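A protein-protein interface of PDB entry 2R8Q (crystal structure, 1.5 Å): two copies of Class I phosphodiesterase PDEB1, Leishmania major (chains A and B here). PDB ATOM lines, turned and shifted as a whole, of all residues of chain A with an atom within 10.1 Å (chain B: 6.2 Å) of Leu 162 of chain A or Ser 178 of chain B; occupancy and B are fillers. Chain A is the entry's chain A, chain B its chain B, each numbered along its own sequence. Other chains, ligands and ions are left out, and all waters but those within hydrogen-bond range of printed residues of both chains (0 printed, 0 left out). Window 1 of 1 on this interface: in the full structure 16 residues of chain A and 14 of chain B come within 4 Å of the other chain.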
ATOM      1  N   ASP A 143      22.604 -24.877  -0.281  1.00  0.00           N
ATOM      2  CA  ASP A 143      22.331 -23.440  -0.244  1.00  0.00           C
ATOM      3  C   ASP A 143      20.915 -23.035  -0.652  1.00  0.00           C
ATOM      4  O   ASP A 143      20.693 -21.937  -1.168  1.00  0.00           O
ATOM      5  CB  ASP A 143      23.380 -22.708  -1.095  1.00  0.00           C
ATOM      6  CG  ASP A 143      23.370 -21.201  -0.887  1.00  0.00           C
ATOM      7  OD1 ASP A 143      23.299 -20.750   0.277  1.00  0.00           O
ATOM      8  OD2 ASP A 143      23.454 -20.465  -1.895  1.00  0.00           O
ATOM      9  N   TYR A 152      11.980 -17.025  -7.884  1.00  0.00           N
ATOM     10  CA  TYR A 152      13.030 -16.285  -8.570  1.00  0.00           C
ATOM     11  C   TYR A 152      12.541 -15.630  -9.854  1.00  0.00           C
ATOM     12  O   TYR A 152      12.975 -14.534 -10.209  1.00  0.00           O
ATOM     13  CB  TYR A 152      14.215 -17.204  -8.864  1.00  0.00           C
ATOM     14  CG  TYR A 152      14.908 -17.677  -7.611  1.00  0.00           C
ATOM     15  CD1 TYR A 152      14.608 -18.917  -7.048  1.00  0.00           C
ATOM     16  CD2 TYR A 152      15.836 -16.866  -6.963  1.00  0.00           C
ATOM     17  CE1 TYR A 152      15.216 -19.336  -5.869  1.00  0.00           C
ATOM     18  CE2 TYR A 152      16.450 -17.273  -5.784  1.00  0.00           C
ATOM     19  CZ  TYR A 152      16.135 -18.508  -5.242  1.00  0.00           C
ATOM     20  OH  TYR A 152      16.736 -18.905  -4.069  1.00  0.00           O
ATOM     21  N   LEU A 153      11.625 -16.299 -10.544  1.00  0.00           N
ATOM     22  CA  LEU A 153      11.085 -15.767 -11.785  1.00  0.00           C
ATOM     23  C   LEU A 153      10.062 -14.664 -11.512  1.00  0.00           C
ATOM     24  O   LEU A 153      10.105 -13.601 -12.130  1.00  0.00           O
ATOM     25  CB  LEU A 153      10.440 -16.893 -12.596  1.00  0.00           C
ATOM     26  CG  LEU A 153      11.366 -18.045 -12.992  1.00  0.00           C
ATOM     27  CD1 LEU A 153      10.576 -19.099 -13.752  1.00  0.00           C
ATOM     28  CD2 LEU A 153      12.512 -17.519 -13.848  1.00  0.00           C
ATOM     29  N   ASP A 156      11.655 -11.213 -10.369  1.00  0.00           N
ATOM     30  CA  ASP A 156      12.720 -10.636 -11.185  1.00  0.00           C
ATOM     31  C   ASP A 156      14.069 -10.682 -10.469  1.00  0.00           C
ATOM     32  O   ASP A 156      14.888  -9.772 -10.607  1.00  0.00           O
ATOM     33  CB  ASP A 156      12.386  -9.184 -11.550  1.00  0.00           C
ATOM     34  CG  ASP A 156      11.260  -9.078 -12.561  1.00  0.00           C
ATOM     35  OD1 ASP A 156      10.142  -9.556 -12.268  1.00  0.00           O
ATOM     36  OD2 ASP A 156      11.493  -8.516 -13.652  1.00  0.00           O
ATOM     37  N   SER A 157      14.294 -11.741  -9.699  1.00  0.00           N
ATOM     38  CA  SER A 157      15.552 -11.906  -8.981  1.00  0.00           C
ATOM     39  C   SER A 157      16.654 -12.124 -10.013  1.00  0.00           C
ATOM     40  O   SER A 157      16.403 -12.662 -11.090  1.00  0.00           O
ATOM     41  CB  SER A 157      15.478 -13.115  -8.049  1.00  0.00           C
ATOM     42  OG  SER A 157      15.241 -14.304  -8.784  1.00  0.00           O
ATOM     43  N   PRO A 158      17.890 -11.699  -9.703  1.00  0.00           N
ATOM     44  CA  PRO A 158      18.994 -11.878 -10.653  1.00  0.00           C
ATOM     45  C   PRO A 158      19.147 -13.327 -11.116  1.00  0.00           C
ATOM     46  O   PRO A 158      19.379 -13.589 -12.298  1.00  0.00           O
ATOM     47  CB  PRO A 158      20.204 -11.387  -9.865  1.00  0.00           C
ATOM     48  CG  PRO A 158      19.613 -10.309  -9.009  1.00  0.00           C
ATOM     49  CD  PRO A 158      18.335 -10.951  -8.516  1.00  0.00           C
ATOM     50  N   LEU A 159      19.025 -14.267 -10.183  1.00  0.00           N
ATOM     51  CA  LEU A 159      19.138 -15.681 -10.523  1.00  0.00           C
ATOM     52  C   LEU A 159      18.046 -16.067 -11.508  1.00  0.00           C
ATOM     53  O   LEU A 159      18.254 -16.907 -12.381  1.00  0.00           O
ATOM     54  CB  LEU A 159      19.021 -16.546  -9.267  1.00  0.00           C
ATOM     55  CG  LEU A 159      20.220 -16.550  -8.318  1.00  0.00           C
ATOM     56  CD1 LEU A 159      19.883 -17.366  -7.082  1.00  0.00           C
ATOM     57  CD2 LEU A 159      21.437 -17.130  -9.027  1.00  0.00           C
ATOM     58  N   GLY A 160      16.878 -15.449 -11.359  1.00  0.00           N
ATOM     59  CA  GLY A 160      15.774 -15.737 -12.254  1.00  0.00           C
ATOM     60  C   GLY A 160      16.042 -15.186 -13.640  1.00  0.00           C
ATOM     61  O   GLY A 160      15.736 -15.828 -14.645  1.00  0.00           O
ATOM     62  N   ILE A 161      16.622 -13.991 -13.692  1.00  0.00           N
ATOM     63  CA  ILE A 161      16.940 -13.340 -14.957  1.00  0.00           C
ATOM     64  C   ILE A 161      17.998 -14.139 -15.719  1.00  0.00           C
ATOM     65  O   ILE A 161      17.913 -14.302 -16.940  1.00  0.00           O
ATOM     66  CB  ILE A 161      17.438 -11.894 -14.710  1.00  0.00           C
ATOM     67  CG1 ILE A 161      16.315 -11.072 -14.065  1.00  0.00           C
ATOM     68  CG2 ILE A 161      17.882 -11.258 -16.022  1.00  0.00           C
ATOM     69  CD1 ILE A 161      16.702  -9.649 -13.705  1.00  0.00           C
ATOM     70  N   LEU A 162      18.992 -14.646 -14.998  1.00  0.00           N
ATOM     71  CA  LEU A 162      20.046 -15.439 -15.623  1.00  0.00           C
ATOM     72  C   LEU A 162      19.442 -16.709 -16.219  1.00  0.00           C
ATOM     73  O   LEU A 162      19.841 -17.153 -17.293  1.00  0.00           O
ATOM     74  CB  LEU A 162      21.126 -15.802 -14.598  1.00  0.00           C
ATOM     75  CG  LEU A 162      22.272 -16.709 -15.065  1.00  0.00           C
ATOM     76  CD1 LEU A 162      22.963 -16.119 -16.295  1.00  0.00           C
ATOM     77  CD2 LEU A 162      23.269 -16.874 -13.927  1.00  0.00           C
ATOM     78  N   SER A 163      18.470 -17.283 -15.518  1.00  0.00           N
ATOM     79  CA  SER A 163      17.808 -18.500 -15.982  1.00  0.00           C
ATOM     80  C   SER A 163      17.070 -18.244 -17.288  1.00  0.00           C
ATOM     81  O   SER A 163      17.118 -19.054 -18.216  1.00  0.00           O
ATOM     82  CB  SER A 163      16.821 -18.994 -14.922  1.00  0.00           C
ATOM     83  OG  SER A 163      17.482 -19.204 -13.687  1.00  0.00           O
ATOM     84  N   SER A 164      16.385 -17.109 -17.352  1.00  0.00           N
ATOM     85  CA  SER A 164      15.635 -16.727 -18.538  1.00  0.00           C
ATOM     86  C   SER A 164      16.577 -16.544 -19.721  1.00  0.00           C
ATOM     87  O   SER A 164      16.273 -16.952 -20.844  1.00  0.00           O
ATOM     88  CB  SER A 164      14.885 -15.421 -18.273  1.00  0.00           C
ATOM     89  OG  SER A 164      14.287 -14.923 -19.454  1.00  0.00           O
ATOM     90  N   ALA A 165      17.727 -15.934 -19.457  1.00  0.00           N
ATOM     91  CA  ALA A 165      18.716 -15.676 -20.496  1.00  0.00           C
ATOM     92  C   ALA A 165      19.538 -16.904 -20.881  1.00  0.00           C
ATOM     93  O   ALA A 165      19.897 -17.071 -22.049  1.00  0.00           O
ATOM     94  CB  ALA A 165      19.646 -14.552 -20.052  1.00  0.00           C
ATOM     95  N   SER A 166      19.835 -17.762 -19.909  1.00  0.00           N
ATOM     96  CA  SER A 166      20.638 -18.954 -20.171  1.00  0.00           C
ATOM     97  C   SER A 166      19.847 -20.077 -20.831  1.00  0.00           C
ATOM     98  O   SER A 166      20.411 -20.896 -21.555  1.00  0.00           O
ATOM     99  CB  SER A 166      21.270 -19.468 -18.873  1.00  0.00           C
ATOM    100  OG  SER A 166      20.276 -19.910 -17.968  1.00  0.00           O
ATOM    101  N   GLY A 167      18.543 -20.120 -20.572  1.00  0.00           N
ATOM    102  CA  GLY A 167      17.711 -21.148 -21.172  1.00  0.00           C
ATOM    103  C   GLY A 167      17.334 -22.306 -20.264  1.00  0.00           C
ATOM    104  O   GLY A 167      16.563 -23.181 -20.661  1.00  0.00           O
ATOM    105  N   ASN A 168      17.869 -22.325 -19.048  1.00  0.00           N
ATOM    106  CA  ASN A 168      17.557 -23.402 -18.112  1.00  0.00           C
ATOM    107  C   ASN A 168      16.641 -22.903 -16.999  1.00  0.00           C
ATOM    108  O   ASN A 168      16.977 -21.962 -16.283  1.00  0.00           O
ATOM    109  CB  ASN A 168      18.846 -23.980 -17.525  1.00  0.00           C
ATOM    110  CG  ASN A 168      18.585 -25.102 -16.546  1.00  0.00           C
ATOM    111  OD1 ASN A 168      18.134 -24.867 -15.426  1.00  0.00           O
ATOM    112  ND2 ASN A 168      18.854 -26.335 -16.968  1.00  0.00           N
ATOM    113  N   ASN A 169      15.486 -23.549 -16.855  1.00  0.00           N
ATOM    114  CA  ASN A 169      14.504 -23.160 -15.851  1.00  0.00           C
ATOM    115  C   ASN A 169      14.719 -23.770 -14.464  1.00  0.00           C
ATOM    116  O   ASN A 169      13.995 -23.445 -13.523  1.00  0.00           O
ATOM    117  CB  ASN A 169      13.097 -23.502 -16.345  1.00  0.00           C
ATOM    118  CG  ASN A 169      12.012 -22.948 -15.442  1.00  0.00           C
ATOM    119  OD1 ASN A 169      11.964 -21.746 -15.179  1.00  0.00           O
ATOM    120  ND2 ASN A 169      11.132 -23.823 -14.965  1.00  0.00           N
ATOM    121  N   SER A 170      15.704 -24.654 -14.335  1.00  0.00           N
ATOM    122  CA  SER A 170      15.988 -25.273 -13.044  1.00  0.00           C
ATOM    123  C   SER A 170      16.993 -24.411 -12.291  1.00  0.00           C
ATOM    124  O   SER A 170      18.142 -24.804 -12.093  1.00  0.00           O
ATOM    125  CB  SER A 170      16.551 -26.683 -13.237  1.00  0.00           C
ATOM    126  OG  SER A 170      15.611 -27.514 -13.898  1.00  0.00           O
ATOM    127  N   VAL A 171      16.532 -23.233 -11.882  1.00  0.00           N
ATOM    128  CA  VAL A 171      17.337 -22.254 -11.160  1.00  0.00           C
ATOM    129  C   VAL A 171      18.110 -22.849  -9.986  1.00  0.00           C
ATOM    130  O   VAL A 171      19.340 -22.799  -9.940  1.00  0.00           O
ATOM    131  CB  VAL A 171      16.445 -21.114 -10.616  1.00  0.00           C
ATOM    132  CG1 VAL A 171      17.306 -20.036  -9.987  1.00  0.00           C
ATOM    133  CG2 VAL A 171      15.581 -20.541 -11.740  1.00  0.00           C
ATOM    134  N   LEU A 172      17.373 -23.406  -9.034  1.00  0.00           N
ATOM    135  CA  LEU A 172      17.968 -23.993  -7.842  1.00  0.00           C
ATOM    136  C   LEU A 172      18.855 -25.203  -8.097  1.00  0.00           C
ATOM    137  O   LEU A 172      19.975 -25.275  -7.591  1.00  0.00           O
ATOM    138  CB  LEU A 172      16.862 -24.392  -6.861  1.00  0.00           C
ATOM    139  CG  LEU A 172      16.206 -23.264  -6.068  1.00  0.00           C
ATOM    140  CD1 LEU A 172      14.848 -23.714  -5.559  1.00  0.00           C
ATOM    141  CD2 LEU A 172      17.114 -22.862  -4.925  1.00  0.00           C
ATOM    142  N   VAL A 174      20.609 -26.247 -10.711  1.00  0.00           N
ATOM    143  CA  VAL A 174      21.913 -26.009 -11.320  1.00  0.00           C
ATOM    144  C   VAL A 174      22.830 -25.415 -10.247  1.00  0.00           C
ATOM    145  O   VAL A 174      24.015 -25.743 -10.180  1.00  0.00           O
ATOM    146  CB  VAL A 174      21.805 -25.044 -12.523  1.00  0.00           C
ATOM    147  CG1 VAL A 174      23.201 -24.661 -13.021  1.00  0.00           C
ATOM    148  CG2 VAL A 174      21.024 -25.715 -13.645  1.00  0.00           C
ATOM    149  N   HIS A 175      22.265 -24.559  -9.397  1.00  0.00           N
ATOM    150  CA  HIS A 175      23.018 -23.937  -8.311  1.00  0.00           C
ATOM    151  C   HIS A 175      23.541 -25.015  -7.361  1.00  0.00           C
ATOM    152  O   HIS A 175      24.702 -24.974  -6.949  1.00  0.00           O
ATOM    153  CB  HIS A 175      22.121 -22.955  -7.546  1.00  0.00           C
ATOM    154  CG  HIS A 175      22.813 -22.228  -6.431  1.00  0.00           C
ATOM    155  ND1 HIS A 175      23.859 -21.355  -6.644  1.00  0.00           N
ATOM    156  CD2 HIS A 175      22.585 -22.221  -5.096  1.00  0.00           C
ATOM    157  CE1 HIS A 175      24.243 -20.839  -5.489  1.00  0.00           C
ATOM    158  NE2 HIS A 175      23.486 -21.349  -4.533  1.00  0.00           N
ATOM    159  N   HIS A 176      22.696 -25.988  -7.018  1.00  0.00           N
ATOM    160  CA  HIS A 176      23.138 -27.048  -6.107  1.00  0.00           C
ATOM    161  C   HIS A 176      24.306 -27.826  -6.728  1.00  0.00           C
ATOM    162  O   HIS A 176      25.263 -28.193  -6.038  1.00  0.00           O
ATOM    163  CB  HIS A 176      21.999 -28.032  -5.784  1.00  0.00           C
ATOM    164  CG  HIS A 176      20.733 -27.384  -5.308  1.00  0.00           C
ATOM    165  ND1 HIS A 176      20.705 -26.384  -4.358  1.00  0.00           N
ATOM    166  CD2 HIS A 176      19.438 -27.652  -5.609  1.00  0.00           C
ATOM    167  CE1 HIS A 176      19.449 -26.065  -4.095  1.00  0.00           C
ATOM    168  NE2 HIS A 176      18.660 -26.820  -4.839  1.00  0.00           N
ATOM    169  N   SER A 178      26.483 -26.709  -8.914  1.00  0.00           N
ATOM    170  CA  SER A 178      27.661 -25.847  -8.904  1.00  0.00           C
ATOM    171  C   SER A 178      28.375 -25.891  -7.560  1.00  0.00           C
ATOM    172  O   SER A 178      29.610 -25.918  -7.500  1.00  0.00           O
ATOM    173  CB  SER A 178      27.261 -24.407  -9.235  1.00  0.00           C
ATOM    174  OG  SER A 178      26.691 -24.330 -10.529  1.00  0.00           O
ATOM    175  N   LEU A 179      27.605 -25.897  -6.475  1.00  0.00           N
ATOM    176  CA  LEU A 179      28.209 -25.951  -5.151  1.00  0.00           C
ATOM    177  C   LEU A 179      28.763 -27.339  -4.848  1.00  0.00           C
ATOM    178  O   LEU A 179      29.749 -27.474  -4.122  1.00  0.00           O
ATOM    179  CB  LEU A 179      27.198 -25.535  -4.082  1.00  0.00           C
ATOM    180  CG  LEU A 179      26.866 -24.041  -4.104  1.00  0.00           C
ATOM    181  CD1 LEU A 179      25.819 -23.733  -3.055  1.00  0.00           C
ATOM    182  CD2 LEU A 179      28.128 -23.230  -3.841  1.00  0.00           C
ATOM    183  N   GLU A 182      32.093 -27.406  -6.300  1.00  0.00           N
ATOM    184  CA  GLU A 182      32.998 -26.602  -5.482  1.00  0.00           C
ATOM    185  C   GLU A 182      33.526 -27.414  -4.300  1.00  0.00           C
ATOM    186  O   GLU A 182      34.732 -27.456  -4.046  1.00  0.00           O
ATOM    187  CB  GLU A 182      32.259 -25.362  -4.973  1.00  0.00           C
ATOM    188  CG  GLU A 182      33.044 -24.524  -3.985  1.00  0.00           C
ATOM    189  CD  GLU A 182      32.220 -23.381  -3.427  1.00  0.00           C
ATOM    190  OE1 GLU A 182      31.782 -22.522  -4.223  1.00  0.00           O
ATOM    191  OE2 GLU A 182      32.007 -23.346  -2.195  1.00  0.00           O
ATOM    192  N   GLU B 173      30.974 -18.389 -19.609  1.00  0.00           N
ATOM    193  CA  GLU B 173      30.143 -17.193 -19.549  1.00  0.00           C
ATOM    194  C   GLU B 173      29.004 -17.256 -18.536  1.00  0.00           C
ATOM    195  O   GLU B 173      28.713 -16.262 -17.868  1.00  0.00           O
ATOM    196  CB  GLU B 173      29.609 -16.855 -20.943  1.00  0.00           C
ATOM    197  CG  GLU B 173      30.694 -16.424 -21.956  1.00  0.00           C
ATOM    198  CD  GLU B 173      31.576 -17.566 -22.443  1.00  0.00           C
ATOM    199  OE1 GLU B 173      31.150 -18.734 -22.367  1.00  0.00           O
ATOM    200  OE2 GLU B 173      32.697 -17.293 -22.926  1.00  0.00           O
ATOM    201  N   VAL B 174      28.348 -18.406 -18.409  1.00  0.00           N
ATOM    202  CA  VAL B 174      27.275 -18.513 -17.424  1.00  0.00           C
ATOM    203  C   VAL B 174      27.907 -18.448 -16.032  1.00  0.00           C
ATOM    204  O   VAL B 174      27.329 -17.881 -15.106  1.00  0.00           O
ATOM    205  CB  VAL B 174      26.489 -19.833 -17.566  1.00  0.00           C
ATOM    206  CG1 VAL B 174      25.507 -19.981 -16.404  1.00  0.00           C
ATOM    207  CG2 VAL B 174      25.735 -19.845 -18.882  1.00  0.00           C
ATOM    208  N   HIS B 175      29.098 -19.029 -15.898  1.00  0.00           N
ATOM    209  CA  HIS B 175      29.830 -19.019 -14.631  1.00  0.00           C
ATOM    210  C   HIS B 175      30.173 -17.575 -14.254  1.00  0.00           C
ATOM    211  O   HIS B 175      30.011 -17.170 -13.100  1.00  0.00           O
ATOM    212  CB  HIS B 175      31.114 -19.850 -14.760  1.00  0.00           C
ATOM    213  CG  HIS B 175      31.939 -19.899 -13.511  1.00  0.00           C
ATOM    214  ND1 HIS B 175      31.469 -20.427 -12.328  1.00  0.00           N
ATOM    215  CD2 HIS B 175      33.207 -19.493 -13.266  1.00  0.00           C
ATOM    216  CE1 HIS B 175      32.414 -20.344 -11.407  1.00  0.00           C
ATOM    217  NE2 HIS B 175      33.478 -19.781 -11.951  1.00  0.00           N
ATOM    218  N   HIS B 176      30.642 -16.797 -15.227  1.00  0.00           N
ATOM    219  CA  HIS B 176      30.985 -15.398 -14.975  1.00  0.00           C
ATOM    220  C   HIS B 176      29.763 -14.631 -14.474  1.00  0.00           C
ATOM    221  O   HIS B 176      29.867 -13.802 -13.564  1.00  0.00           O
ATOM    222  CB  HIS B 176      31.504 -14.720 -16.248  1.00  0.00           C
ATOM    223  CG  HIS B 176      32.687 -15.400 -16.866  1.00  0.00           C
ATOM    224  ND1 HIS B 176      33.707 -15.953 -16.122  1.00  0.00           N
ATOM    225  CD2 HIS B 176      33.025 -15.585 -18.165  1.00  0.00           C
ATOM    226  CE1 HIS B 176      34.624 -16.449 -16.936  1.00  0.00           C
ATOM    227  NE2 HIS B 176      34.234 -16.236 -18.181  1.00  0.00           N
ATOM    228  N   CYS B 177      28.607 -14.903 -15.077  1.00  0.00           N
ATOM    229  CA  CYS B 177      27.368 -14.239 -14.682  1.00  0.00           C
ATOM    230  C   CYS B 177      26.993 -14.595 -13.248  1.00  0.00           C
ATOM    231  O   CYS B 177      26.599 -13.731 -12.469  1.00  0.00           O
ATOM    232  CB  CYS B 177      26.217 -14.639 -15.610  1.00  0.00           C
ATOM    233  SG  CYS B 177      26.282 -13.930 -17.266  1.00  0.00           S
ATOM    234  N   SER B 178      27.112 -15.873 -12.908  1.00  0.00           N
ATOM    235  CA  SER B 178      26.777 -16.332 -11.566  1.00  0.00           C
ATOM    236  C   SER B 178      27.611 -15.624 -10.504  1.00  0.00           C
ATOM    237  O   SER B 178      27.093 -15.241  -9.453  1.00  0.00           O
ATOM    238  CB  SER B 178      26.981 -17.845 -11.459  1.00  0.00           C
ATOM    239  OG  SER B 178      26.066 -18.534 -12.291  1.00  0.00           O
ATOM    240  N   LEU B 179      28.900 -15.455 -10.774  1.00  0.00           N
ATOM    241  CA  LEU B 179      29.779 -14.786  -9.821  1.00  0.00           C
ATOM    242  C   LEU B 179      29.503 -13.290  -9.782  1.00  0.00           C
ATOM    243  O   LEU B 179      29.660 -12.654  -8.740  1.00  0.00           O
ATOM    244  CB  LEU B 179      31.247 -15.050 -10.162  1.00  0.00           C
ATOM    245  CG  LEU B 179      31.709 -16.495  -9.957  1.00  0.00           C
ATOM    246  CD1 LEU B 179      33.180 -16.616 -10.314  1.00  0.00           C
ATOM    247  CD2 LEU B 179      31.470 -16.914  -8.515  1.00  0.00           C
ATOM    248  N   ALA B 180      29.089 -12.726 -10.914  1.00  0.00           N
ATOM    249  CA  ALA B 180      28.765 -11.304 -10.972  1.00  0.00           C
ATOM    250  C   ALA B 180      27.583 -11.058 -10.038  1.00  0.00           C
ATOM    251  O   ALA B 180      27.560 -10.091  -9.276  1.00  0.00           O
ATOM    252  CB  ALA B 180      28.398 -10.897 -12.400  1.00  0.00           C
ATOM    253  N   ILE B 181      26.600 -11.949 -10.109  1.00  0.00           N
ATOM    254  CA  ILE B 181      25.411 -11.854  -9.272  1.00  0.00           C
ATOM    255  C   ILE B 181      25.789 -11.982  -7.801  1.00  0.00           C
ATOM    256  O   ILE B 181      25.244 -11.280  -6.950  1.00  0.00           O
ATOM    257  CB  ILE B 181      24.393 -12.960  -9.648  1.00  0.00           C
ATOM    258  CG1 ILE B 181      23.790 -12.647 -11.020  1.00  0.00           C
ATOM    259  CG2 ILE B 181      23.306 -13.076  -8.585  1.00  0.00           C
ATOM    260  CD1 ILE B 181      22.938 -13.761 -11.582  1.00  0.00           C
ATOM    261  N   GLU B 182      26.732 -12.872  -7.509  1.00  0.00           N
ATOM    262  CA  GLU B 182      27.185 -13.091  -6.139  1.00  0.00           C
ATOM    263  C   GLU B 182      27.818 -11.827  -5.561  1.00  0.00           C
ATOM    264  O   GLU B 182      27.523 -11.428  -4.431  1.00  0.00           O
ATOM    265  CB  GLU B 182      28.196 -14.237  -6.106  1.00  0.00           C
ATOM    266  CG  GLU B 182      28.716 -14.573  -4.721  1.00  0.00           C
ATOM    267  CD  GLU B 182      29.844 -15.579  -4.762  1.00  0.00           C
ATOM    268  OE1 GLU B 182      29.668 -16.643  -5.393  1.00  0.00           O
ATOM    269  OE2 GLU B 182      30.907 -15.306  -4.163  1.00  0.00           O
ATOM    270  N   ILE B 183      28.693 -11.203  -6.340  1.00  0.00           N
ATOM    271  CA  ILE B 183      29.371  -9.983  -5.916  1.00  0.00           C
ATOM    272  C   ILE B 183      28.377  -8.852  -5.655  1.00  0.00           C
ATOM    273  O   ILE B 183      28.437  -8.183  -4.618  1.00  0.00           O
ATOM    274  CB  ILE B 183      30.384  -9.519  -6.991  1.00  0.00           C
ATOM    275  CG1 ILE B 183      31.535 -10.523  -7.083  1.00  0.00           C
ATOM    276  CG2 ILE B 183      30.909  -8.124  -6.661  1.00  0.00           C
ATOM    277  CD1 ILE B 183      32.536 -10.208  -8.177  1.00  0.00           C
ATOM    278  N   ILE B 208      23.886  -9.412 -18.002  1.00  0.00           N
ATOM    279  CA  ILE B 208      23.908 -10.822 -18.354  1.00  0.00           C
ATOM    280  C   ILE B 208      23.943 -11.020 -19.872  1.00  0.00           C
ATOM    281  O   ILE B 208      24.723 -11.834 -20.370  1.00  0.00           O
ATOM    282  CB  ILE B 208      22.689 -11.541 -17.734  1.00  0.00           C
ATOM    283  CG1 ILE B 208      22.838 -11.544 -16.207  1.00  0.00           C
ATOM    284  CG2 ILE B 208      22.572 -12.959 -18.284  1.00  0.00           C
ATOM    285  CD1 ILE B 208      21.588 -11.966 -15.437  1.00  0.00           C
ATOM    286  N   LEU B 212      27.041 -13.014 -21.719  1.00  0.00           N
ATOM    287  CA  LEU B 212      26.770 -14.193 -22.537  1.00  0.00           C
ATOM    288  C   LEU B 212      27.182 -13.990 -23.991  1.00  0.00           C
ATOM    289  O   LEU B 212      27.553 -14.944 -24.667  1.00  0.00           O
ATOM    290  CB  LEU B 212      25.285 -14.569 -22.465  1.00  0.00           C
ATOM    291  CG  LEU B 212      24.802 -15.005 -21.077  1.00  0.00           C
ATOM    292  CD1 LEU B 212      23.322 -15.347 -21.138  1.00  0.00           C
ATOM    293  CD2 LEU B 212      25.611 -16.208 -20.596  1.00  0.00           C
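O of Leu 162 of chain A lies within hydrogen-bond range of OG of Ser 166 of chain A (2.9 Å).
O of Glu 173 of chain B sits at hydrogen-bond distance from SG of Cys 177 of chain B, 3.4 Å away.
The side-chain hydroxyl (OG) of Ser 178 of chain B lies within hydrogen-bond range of the backbone carbonyl oxygen (O) of Val 174 of chain B (3.2 Å).
Among the printed residues, merely in contact across the chains: Pro 158 of chain A with Ile 181 of chain B (3.6 Å), Ile 161 of chain A with Ile 208 of chain B (3.8 Å), Leu 162 of chain A with Cys 177 of chain B (3.6 Å), Leu 162 of chain A with Ser 178 of chain B (3.6 Å), Leu 162 of chain A with Ile 181 of chain B (3.9 Å), Leu 162 of chain A with Ile 208 of chain B (3.8 Å), Ala 165 of chain A with Ile 208 of chain B (3.8 Å) and Ala 165 of chain A with Leu 212 of chain B (3.9 Å).
Of chain B, only Cys 177, Ser 178, Ile 181 and Ile 208 come within 4 Å of Leu 162 of chain A.
Of chain A, only Leu 162 (3.6 Å) comes within 4 Å of Ser 178 of chain B.
Of chain A, only Leu 162 comes within 4 Å of Cys 177 of chain B.
No residue of chain A comes within 4 Å of Ala 180 of chain B.
Ile 181 of chain B touches just these residues of chain A: Pro 158 (3.6 Å) and Leu 162 (3.9 Å).
Of the printed residues of chain B, Pro 158 of chain A touches Ile 181.
Of the printed residues of chain B, Ile 161 of chain A touches Ile 208.
Of the printed residues of chain B, Ala 165 of chain A touches Ile 208 and Leu 212.
Gly 160 of chain A touches none of the printed residues of chain B.
Ile 183 of chain B touches none of the printed residues of chain A.
The nearest residue of chain B that does not touch Leu 162 of chain A is Val 174 of chain B (4.3 Å).
The nearest residue of chain A that does not touch Ser 178 of chain B is Leu 159 of chain A (5.8 Å).
Of the 13 printed residues of chain B, 5 touch a printed residue of chain A.
Printed residues of chain B that touch a printed residue of chain A: Cys 177, Ser 178, Ile 181, Ile 208 and Leu 212.
Hydrophobic or aromatic side chains of chain A within 4 Å of the printed part of chain B: Pro 158, Ile 161, Leu 162 and Ala 165.
Among the printed residues, no Asp or Glu carboxylate lies within 4 Å of a Lys or Arg side-chain nitrogen of the other chain.
Positions printed for both chains: 174, 175, 176, 178, 179 and 182.
Of the 8 pairs that touch across the chains among the printed residues, none has its exchanged pair printed and touching as well.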
